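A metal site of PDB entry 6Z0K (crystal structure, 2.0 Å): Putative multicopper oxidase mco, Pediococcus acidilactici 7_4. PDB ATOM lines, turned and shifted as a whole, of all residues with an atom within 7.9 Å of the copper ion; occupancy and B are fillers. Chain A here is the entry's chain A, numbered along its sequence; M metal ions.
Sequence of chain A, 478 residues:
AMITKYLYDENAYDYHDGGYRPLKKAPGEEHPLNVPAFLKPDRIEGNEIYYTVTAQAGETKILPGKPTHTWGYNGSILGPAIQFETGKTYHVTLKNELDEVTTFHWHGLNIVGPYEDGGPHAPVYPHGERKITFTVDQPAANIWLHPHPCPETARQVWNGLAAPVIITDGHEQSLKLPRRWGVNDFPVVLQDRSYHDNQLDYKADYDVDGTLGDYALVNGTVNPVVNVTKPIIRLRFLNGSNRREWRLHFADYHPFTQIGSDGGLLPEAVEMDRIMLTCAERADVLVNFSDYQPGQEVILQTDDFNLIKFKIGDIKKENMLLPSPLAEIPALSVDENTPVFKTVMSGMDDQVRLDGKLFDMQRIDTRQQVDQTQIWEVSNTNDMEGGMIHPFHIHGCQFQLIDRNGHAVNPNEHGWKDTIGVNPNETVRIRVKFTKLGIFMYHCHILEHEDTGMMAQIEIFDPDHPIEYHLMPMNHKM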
ATOM      1  N   ASP A 209      14.325  24.679  -1.730  1.00  0.00           N
ATOM      2  CA  ASP A 209      13.029  25.395  -1.618  1.00  0.00           C
ATOM      3  C   ASP A 209      12.016  24.874  -2.648  1.00  0.00           C
ATOM      4  O   ASP A 209      10.912  25.427  -2.715  1.00  0.00           O
ATOM      5  CB  ASP A 209      13.216  26.904  -1.795  1.00  0.00           C
ATOM      6  CG  ASP A 209      12.182  27.741  -1.061  1.00  0.00           C
ATOM      7  OD1 ASP A 209      11.613  27.252  -0.070  1.00  0.00           O
ATOM      8  OD2 ASP A 209      11.950  28.886  -1.496  1.00  0.00           O
ATOM      9  N   ARG A 243       7.370  21.686  -7.288  1.00  0.00           N
ATOM     10  CA  ARG A 243       7.085  22.988  -6.621  1.00  0.00           C
ATOM     11  C   ARG A 243       6.235  23.934  -7.468  1.00  0.00           C
ATOM     12  O   ARG A 243       5.455  24.692  -6.873  1.00  0.00           O
ATOM     13  CB  ARG A 243       8.403  23.696  -6.261  1.00  0.00           C
ATOM     14  CG  ARG A 243       8.217  24.951  -5.408  1.00  0.00           C
ATOM     15  CD  ARG A 243       8.282  26.239  -6.205  1.00  0.00           C
ATOM     16  NE  ARG A 243       8.016  27.414  -5.382  1.00  0.00           N
ATOM     17  CZ  ARG A 243       6.819  27.824  -4.970  1.00  0.00           C
ATOM     18  NH1 ARG A 243       6.710  28.922  -4.227  1.00  0.00           N
ATOM     19  NH2 ARG A 243       5.718  27.153  -5.293  1.00  0.00           N
ATOM     20  N   MET A 345       2.675  25.614   9.707  1.00  0.00           N
ATOM     21  CA  MET A 345       3.760  25.527   8.707  1.00  0.00           C
ATOM     22  C   MET A 345       4.582  26.809   8.834  1.00  0.00           C
ATOM     23  O   MET A 345       3.982  27.905   8.774  1.00  0.00           O
ATOM     24  CB  MET A 345       3.189  25.411   7.297  1.00  0.00           C
ATOM     25  CG  MET A 345       2.245  24.243   7.132  1.00  0.00           C
ATOM     26  SD  MET A 345       1.630  24.143   5.443  1.00  0.00           S
ATOM     27  CE  MET A 345       2.962  23.197   4.715  1.00  0.00           C
ATOM     28  N   SER A 346       5.893  26.677   9.000  1.00  0.00           N
ATOM     29  CA  SER A 346       6.807  27.819   9.190  1.00  0.00           C
ATOM     30  C   SER A 346       8.080  27.632   8.370  1.00  0.00           C
ATOM     31  O   SER A 346       8.431  26.483   8.049  1.00  0.00           O
ATOM     32  CB  SER A 346       7.122  28.026  10.650  1.00  0.00           C
ATOM     33  OG  SER A 346       7.824  26.905  11.167  1.00  0.00           O
ATOM     34  N   GLY A 347       8.731  28.748   8.064  1.00  0.00           N
ATOM     35  CA  GLY A 347      10.050  28.768   7.432  1.00  0.00           C
ATOM     36  C   GLY A 347       9.983  28.474   5.943  1.00  0.00           C
ATOM     37  O   GLY A 347       8.882  28.192   5.421  1.00  0.00           O
ATOM     38  N   MET A 348      11.143  28.584   5.302  1.00  0.00           N
ATOM     39  CA  MET A 348      11.346  28.266   3.873  1.00  0.00           C
ATOM     40  C   MET A 348      12.717  27.595   3.743  1.00  0.00           C
ATOM     41  O   MET A 348      13.462  27.549   4.747  1.00  0.00           O
ATOM     42  CB  MET A 348      11.293  29.534   3.031  1.00  0.00           C
ATOM     43  CG  MET A 348       9.911  30.155   2.951  1.00  0.00           C
ATOM     44  SD  MET A 348       9.822  31.770   2.110  1.00  0.00           S
ATOM     45  CE  MET A 348      10.822  31.477   0.641  1.00  0.00           C
ATOM     46  N   ASP A 349      13.016  27.088   2.547  1.00  0.00           N
ATOM     47  CA  ASP A 349      14.336  26.477   2.243  1.00  0.00           C
ATOM     48  C   ASP A 349      14.579  25.331   3.233  1.00  0.00           C
ATOM     49  O   ASP A 349      13.629  24.555   3.491  1.00  0.00           O
ATOM     50  CB  ASP A 349      15.431  27.542   2.272  1.00  0.00           C
ATOM     51  CG  ASP A 349      15.100  28.754   1.421  1.00  0.00           C
ATOM     52  OD1 ASP A 349      15.077  28.616   0.184  1.00  0.00           O
ATOM     53  OD2 ASP A 349      14.847  29.826   2.001  1.00  0.00           O
ATOM     54  N   VAL A 352      12.279  24.858   6.844  1.00  0.00           N
ATOM     55  CA  VAL A 352      10.837  24.467   6.892  1.00  0.00           C
ATOM     56  C   VAL A 352      10.603  23.574   8.103  1.00  0.00           C
ATOM     57  O   VAL A 352      11.423  22.673   8.360  1.00  0.00           O
ATOM     58  CB  VAL A 352      10.346  23.795   5.602  1.00  0.00           C
ATOM     59  CG1 VAL A 352      10.329  24.786   4.446  1.00  0.00           C
ATOM     60  CG2 VAL A 352      11.128  22.536   5.249  1.00  0.00           C
ATOM     61  N   ARG A 353       9.516  23.837   8.830  1.00  0.00           N
ATOM     62  CA  ARG A 353       9.114  23.019  10.005  1.00  0.00           C
ATOM     63  C   ARG A 353       7.589  22.912  10.048  1.00  0.00           C
ATOM     64  O   ARG A 353       6.901  23.855   9.606  1.00  0.00           O
ATOM     65  CB  ARG A 353       9.634  23.641  11.309  1.00  0.00           C
ATOM     66  CG  ARG A 353      11.150  23.716  11.426  1.00  0.00           C
ATOM     67  CD  ARG A 353      11.812  22.358  11.563  1.00  0.00           C
ATOM     68  NE  ARG A 353      13.255  22.449  11.790  1.00  0.00           N
ATOM     69  CZ  ARG A 353      14.186  22.680  10.870  1.00  0.00           C
ATOM     70  NH1 ARG A 353      13.855  22.864   9.599  1.00  0.00           N
ATOM     71  NH2 ARG A 353      15.456  22.748  11.225  1.00  0.00           N
ATOM     72  N   ASN A 380       0.131  29.180   7.931  1.00  0.00           N
ATOM     73  CA  ASN A 380       1.421  29.475   7.268  1.00  0.00           C
ATOM     74  C   ASN A 380       1.940  30.781   7.858  1.00  0.00           C
ATOM     75  O   ASN A 380       1.321  31.830   7.593  1.00  0.00           O
ATOM     76  CB  ASN A 380       1.244  29.557   5.745  1.00  0.00           C
ATOM     77  CG  ASN A 380       2.495  30.015   5.013  1.00  0.00           C
ATOM     78  OD1 ASN A 380       3.545  30.238   5.621  1.00  0.00           O
ATOM     79  ND2 ASN A 380       2.384  30.132   3.698  1.00  0.00           N
ATOM     80  N   ASN A 382       4.776  32.263   7.222  1.00  0.00           N
ATOM     81  CA  ASN A 382       5.658  33.011   6.294  1.00  0.00           C
ATOM     82  C   ASN A 382       5.169  34.458   6.214  1.00  0.00           C
ATOM     83  O   ASN A 382       3.939  34.697   6.342  1.00  0.00           O
ATOM     84  CB  ASN A 382       5.706  32.419   4.890  1.00  0.00           C
ATOM     85  CG  ASN A 382       6.472  31.120   4.809  1.00  0.00           C
ATOM     86  OD1 ASN A 382       6.854  30.529   5.819  1.00  0.00           O
ATOM     87  ND2 ASN A 382       6.693  30.652   3.586  1.00  0.00           N
ATOM     88  N   MET A 388       5.613  32.441   0.756  1.00  0.00           N
ATOM     89  CA  MET A 388       5.471  31.252  -0.112  1.00  0.00           C
ATOM     90  C   MET A 388       4.121  30.609   0.177  1.00  0.00           C
ATOM     91  O   MET A 388       3.745  30.554   1.357  1.00  0.00           O
ATOM     92  CB  MET A 388       6.584  30.295   0.297  1.00  0.00           C
ATOM     93  CG  MET A 388       6.998  29.336  -0.754  1.00  0.00           C
ATOM     94  SD  MET A 388       8.438  28.453  -0.126  1.00  0.00           S
ATOM     95  CE  MET A 388       8.740  27.449  -1.575  1.00  0.00           C
ATOM     96  N   ILE A 389       3.418  30.163  -0.862  1.00  0.00           N
ATOM     97  CA  ILE A 389       2.177  29.356  -0.686  1.00  0.00           C
ATOM     98  C   ILE A 389       2.586  27.902  -0.518  1.00  0.00           C
ATOM     99  O   ILE A 389       3.173  27.322  -1.461  1.00  0.00           O
ATOM    100  CB  ILE A 389       1.198  29.535  -1.866  1.00  0.00           C
ATOM    101  CG1 ILE A 389       0.829  31.006  -2.058  1.00  0.00           C
ATOM    102  CG2 ILE A 389      -0.044  28.679  -1.667  1.00  0.00           C
ATOM    103  CD1 ILE A 389       0.347  31.338  -3.455  1.00  0.00           C
ATOM    104  N   HIS A 390       2.289  27.327   0.644  1.00  0.00           N
ATOM    105  CA  HIS A 390       2.568  25.901   0.966  1.00  0.00           C
ATOM    106  C   HIS A 390       1.300  25.090   0.721  1.00  0.00           C
ATOM    107  O   HIS A 390       0.291  25.318   1.375  1.00  0.00           O
ATOM    108  CB  HIS A 390       3.020  25.721   2.412  1.00  0.00           C
ATOM    109  CG  HIS A 390       4.344  26.335   2.731  1.00  0.00           C
ATOM    110  ND1 HIS A 390       5.525  25.634   2.623  1.00  0.00           N
ATOM    111  CD2 HIS A 390       4.667  27.565   3.179  1.00  0.00           C
ATOM    112  CE1 HIS A 390       6.527  26.414   2.985  1.00  0.00           C
ATOM    113  NE2 HIS A 390       6.023  27.603   3.333  1.00  0.00           N
ATOM    114  N   PRO A 391       1.326  24.115  -0.223  1.00  0.00           N
ATOM    115  CA  PRO A 391       0.193  23.217  -0.420  1.00  0.00           C
ATOM    116  C   PRO A 391       0.151  22.129   0.651  1.00  0.00           C
ATOM    117  O   PRO A 391       0.976  21.232   0.617  1.00  0.00           O
ATOM    118  CB  PRO A 391       0.414  22.634  -1.821  1.00  0.00           C
ATOM    119  CG  PRO A 391       1.919  22.693  -2.011  1.00  0.00           C
ATOM    120  CD  PRO A 391       2.404  23.872  -1.192  1.00  0.00           C
ATOM    121  N   PHE A 392      -0.801  22.248   1.572  1.00  0.00           N
ATOM    122  CA  PHE A 392      -0.944  21.349   2.737  1.00  0.00           C
ATOM    123  C   PHE A 392      -1.826  20.158   2.369  1.00  0.00           C
ATOM    124  O   PHE A 392      -2.926  20.379   1.824  1.00  0.00           O
ATOM    125  CB  PHE A 392      -1.542  22.125   3.900  1.00  0.00           C
ATOM    126  CG  PHE A 392      -1.692  21.319   5.163  1.00  0.00           C
ATOM    127  CD1 PHE A 392      -0.603  21.118   5.995  1.00  0.00           C
ATOM    128  CD2 PHE A 392      -2.916  20.768   5.512  1.00  0.00           C
ATOM    129  CE1 PHE A 392      -0.747  20.373   7.158  1.00  0.00           C
ATOM    130  CE2 PHE A 392      -3.046  20.027   6.674  1.00  0.00           C
ATOM    131  CZ  PHE A 392      -1.959  19.833   7.500  1.00  0.00           C
ATOM    132  N   HIS A 443       1.460  16.906   5.552  1.00  0.00           N
ATOM    133  CA  HIS A 443       2.705  17.591   5.130  1.00  0.00           C
ATOM    134  C   HIS A 443       2.431  18.624   4.048  1.00  0.00           C
ATOM    135  O   HIS A 443       1.334  18.634   3.460  1.00  0.00           O
ATOM    136  CB  HIS A 443       3.712  16.557   4.610  1.00  0.00           C
ATOM    137  CG  HIS A 443       3.217  15.734   3.473  1.00  0.00           C
ATOM    138  ND1 HIS A 443       3.496  16.054   2.155  1.00  0.00           N
ATOM    139  CD2 HIS A 443       2.479  14.610   3.442  1.00  0.00           C
ATOM    140  CE1 HIS A 443       2.950  15.158   1.367  1.00  0.00           C
ATOM    141  NE2 HIS A 443       2.315  14.257   2.125  1.00  0.00           N
ATOM    142  N   CYS A 444       3.453  19.429   3.813  1.00  0.00           N
ATOM    143  CA  CYS A 444       3.564  20.288   2.617  1.00  0.00           C
ATOM    144  C   CYS A 444       3.800  19.392   1.402  1.00  0.00           C
ATOM    145  O   CYS A 444       4.630  18.464   1.512  1.00  0.00           O
ATOM    146  CB  CYS A 444       4.734  21.240   2.728  1.00  0.00           C
ATOM    147  SG  CYS A 444       4.830  22.341   1.303  1.00  0.00           S
ATOM    148  N   HIS A 445       3.143  19.673   0.281  1.00  0.00           N
ATOM    149  CA  HIS A 445       3.301  18.868  -0.951  1.00  0.00           C
ATOM    150  C   HIS A 445       4.273  19.514  -1.937  1.00  0.00           C
ATOM    151  O   HIS A 445       4.357  19.030  -3.078  1.00  0.00           O
ATOM    152  CB  HIS A 445       1.954  18.580  -1.615  1.00  0.00           C
ATOM    153  CG  HIS A 445       1.938  17.250  -2.283  1.00  0.00           C
ATOM    154  ND1 HIS A 445       2.587  17.029  -3.489  1.00  0.00           N
ATOM    155  CD2 HIS A 445       1.400  16.069  -1.916  1.00  0.00           C
ATOM    156  CE1 HIS A 445       2.420  15.764  -3.843  1.00  0.00           C
ATOM    157  NE2 HIS A 445       1.707  15.166  -2.894  1.00  0.00           N
ATOM    158  N   ILE A 446       5.006  20.556  -1.536  1.00  0.00           N
ATOM    159  CA  ILE A 446       6.272  20.912  -2.231  1.00  0.00           C
ATOM    160  C   ILE A 446       7.253  19.802  -1.839  1.00  0.00           C
ATOM    161  O   ILE A 446       7.638  19.741  -0.662  1.00  0.00           O
ATOM    162  CB  ILE A 446       6.765  22.323  -1.877  1.00  0.00           C
ATOM    163  CG1 ILE A 446       5.796  23.374  -2.436  1.00  0.00           C
ATOM    164  CG2 ILE A 446       8.182  22.550  -2.396  1.00  0.00           C
ATOM    165  CD1 ILE A 446       5.943  24.741  -1.810  1.00  0.00           C
ATOM    166  N   LEU A 447       7.606  18.941  -2.802  1.00  0.00           N
ATOM    167  CA  LEU A 447       8.238  17.623  -2.497  1.00  0.00           C
ATOM    168  C   LEU A 447       9.594  17.802  -1.801  1.00  0.00           C
ATOM    169  O   LEU A 447       9.929  16.930  -0.980  1.00  0.00           O
ATOM    170  CB  LEU A 447       8.343  16.802  -3.788  1.00  0.00           C
ATOM    171  CG  LEU A 447       7.013  16.431  -4.440  1.00  0.00           C
ATOM    172  CD1 LEU A 447       7.245  15.653  -5.723  1.00  0.00           C
ATOM    173  CD2 LEU A 447       6.118  15.622  -3.499  1.00  0.00           C
ATOM    174  N   GLU A 448      10.333  18.868  -2.096  1.00  0.00           N
ATOM    175  CA  GLU A 448      11.650  19.134  -1.431  1.00  0.00           C
ATOM    176  C   GLU A 448      11.423  19.528   0.040  1.00  0.00           C
ATOM    177  O   GLU A 448      12.264  19.141   0.882  1.00  0.00           O
ATOM    178  CB  GLU A 448      12.447  20.210  -2.172  1.00  0.00           C
ATOM    179  CG  GLU A 448      13.134  19.689  -3.420  1.00  0.00           C
ATOM    180  CD  GLU A 448      12.249  19.474  -4.638  1.00  0.00           C
ATOM    181  OE1 GLU A 448      11.101  19.994  -4.640  1.00  0.00           O
ATOM    182  OE2 GLU A 448      12.690  18.791  -5.589  1.00  0.00           O
ATOM    183  N   HIS A 449      10.343  20.248   0.344  1.00  0.00           N
ATOM    184  CA  HIS A 449       9.944  20.582   1.742  1.00  0.00           C
ATOM    185  C   HIS A 449       9.574  19.306   2.492  1.00  0.00           C
ATOM    186  O   HIS A 449      10.030  19.129   3.647  1.00  0.00           O
ATOM    187  CB  HIS A 449       8.788  21.582   1.756  1.00  0.00           C
ATOM    188  CG  HIS A 449       9.171  22.946   1.299  1.00  0.00           C
ATOM    189  ND1 HIS A 449       8.328  24.028   1.426  1.00  0.00           N
ATOM    190  CD2 HIS A 449      10.310  23.423   0.751  1.00  0.00           C
ATOM    191  CE1 HIS A 449       8.913  25.105   0.952  1.00  0.00           C
ATOM    192  NE2 HIS A 449      10.142  24.761   0.540  1.00  0.00           N
ATOM    193  N   GLU A 450       8.770  18.447   1.859  1.00  0.00           N
ATOM    194  CA  GLU A 450       8.381  17.123   2.404  1.00  0.00           C
ATOM    195  C   GLU A 450       9.646  16.333   2.737  1.00  0.00           C
ATOM    196  O   GLU A 450       9.753  15.839   3.883  1.00  0.00           O
ATOM    197  CB  GLU A 450       7.515  16.403   1.361  1.00  0.00           C
ATOM    198  CG  GLU A 450       7.076  15.010   1.759  1.00  0.00           C
ATOM    199  CD  GLU A 450       6.541  14.229   0.573  1.00  0.00           C
ATOM    200  OE1 GLU A 450       6.853  13.019   0.479  1.00  0.00           O
ATOM    201  OE2 GLU A 450       5.823  14.822  -0.252  1.00  0.00           O
ATOM    202  N   MET A 454       9.215  18.551   6.405  1.00  0.00           N
ATOM    203  CA  MET A 454       7.984  19.336   6.687  1.00  0.00           C
ATOM    204  C   MET A 454       6.780  18.396   6.613  1.00  0.00           C
ATOM    205  O   MET A 454       5.932  18.560   5.717  1.00  0.00           O
ATOM    206  CB  MET A 454       7.833  20.496   5.700  1.00  0.00           C
ATOM    207  CG  MET A 454       6.869  21.565   6.171  1.00  0.00           C
ATOM    208  SD  MET A 454       6.763  22.959   5.019  1.00  0.00           S
ATOM    209  CE  MET A 454       6.459  24.265   6.209  1.00  0.00           C
HETATM  210 CU    CU M   1       6.169  23.838   1.945  1.00  0.00          CU
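The copper ion is bound by a ring nitrogen (ND1) of His 390, the side-chain sulfur of Cys 444 and a ring nitrogen (ND1) of His 449. The copper ion has three donor atoms within binding distance.
Ile 446 touches the copper ion. Met 454 touches the copper ion (SD to CU, 3.3 Å). The nearest printed residue that does not touch the copper ion is Met 345 (4.3 Å).
O of His 449 sits at hydrogen-bond distance from N of Met 454. O of Met 454 is in hydrogen-bond range of N of Cys 444 (3.2 Å). The side-chain sulfur (SG) of Cys 444 sits close to the backbone NH (N) of Ile 446 (3.4 Å). ND2 of Asn 382 sits at hydrogen-bond distance from NE2 of His 390. A ring nitrogen (NE2) of His 449 is in hydrogen-bond range of the side-chain carboxylate (OD1) of Asp 209 (3.0 Å). A ring nitrogen (ND1) of His 390 lies close to the side-chain sulfur of Met 454 (3.8 Å).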
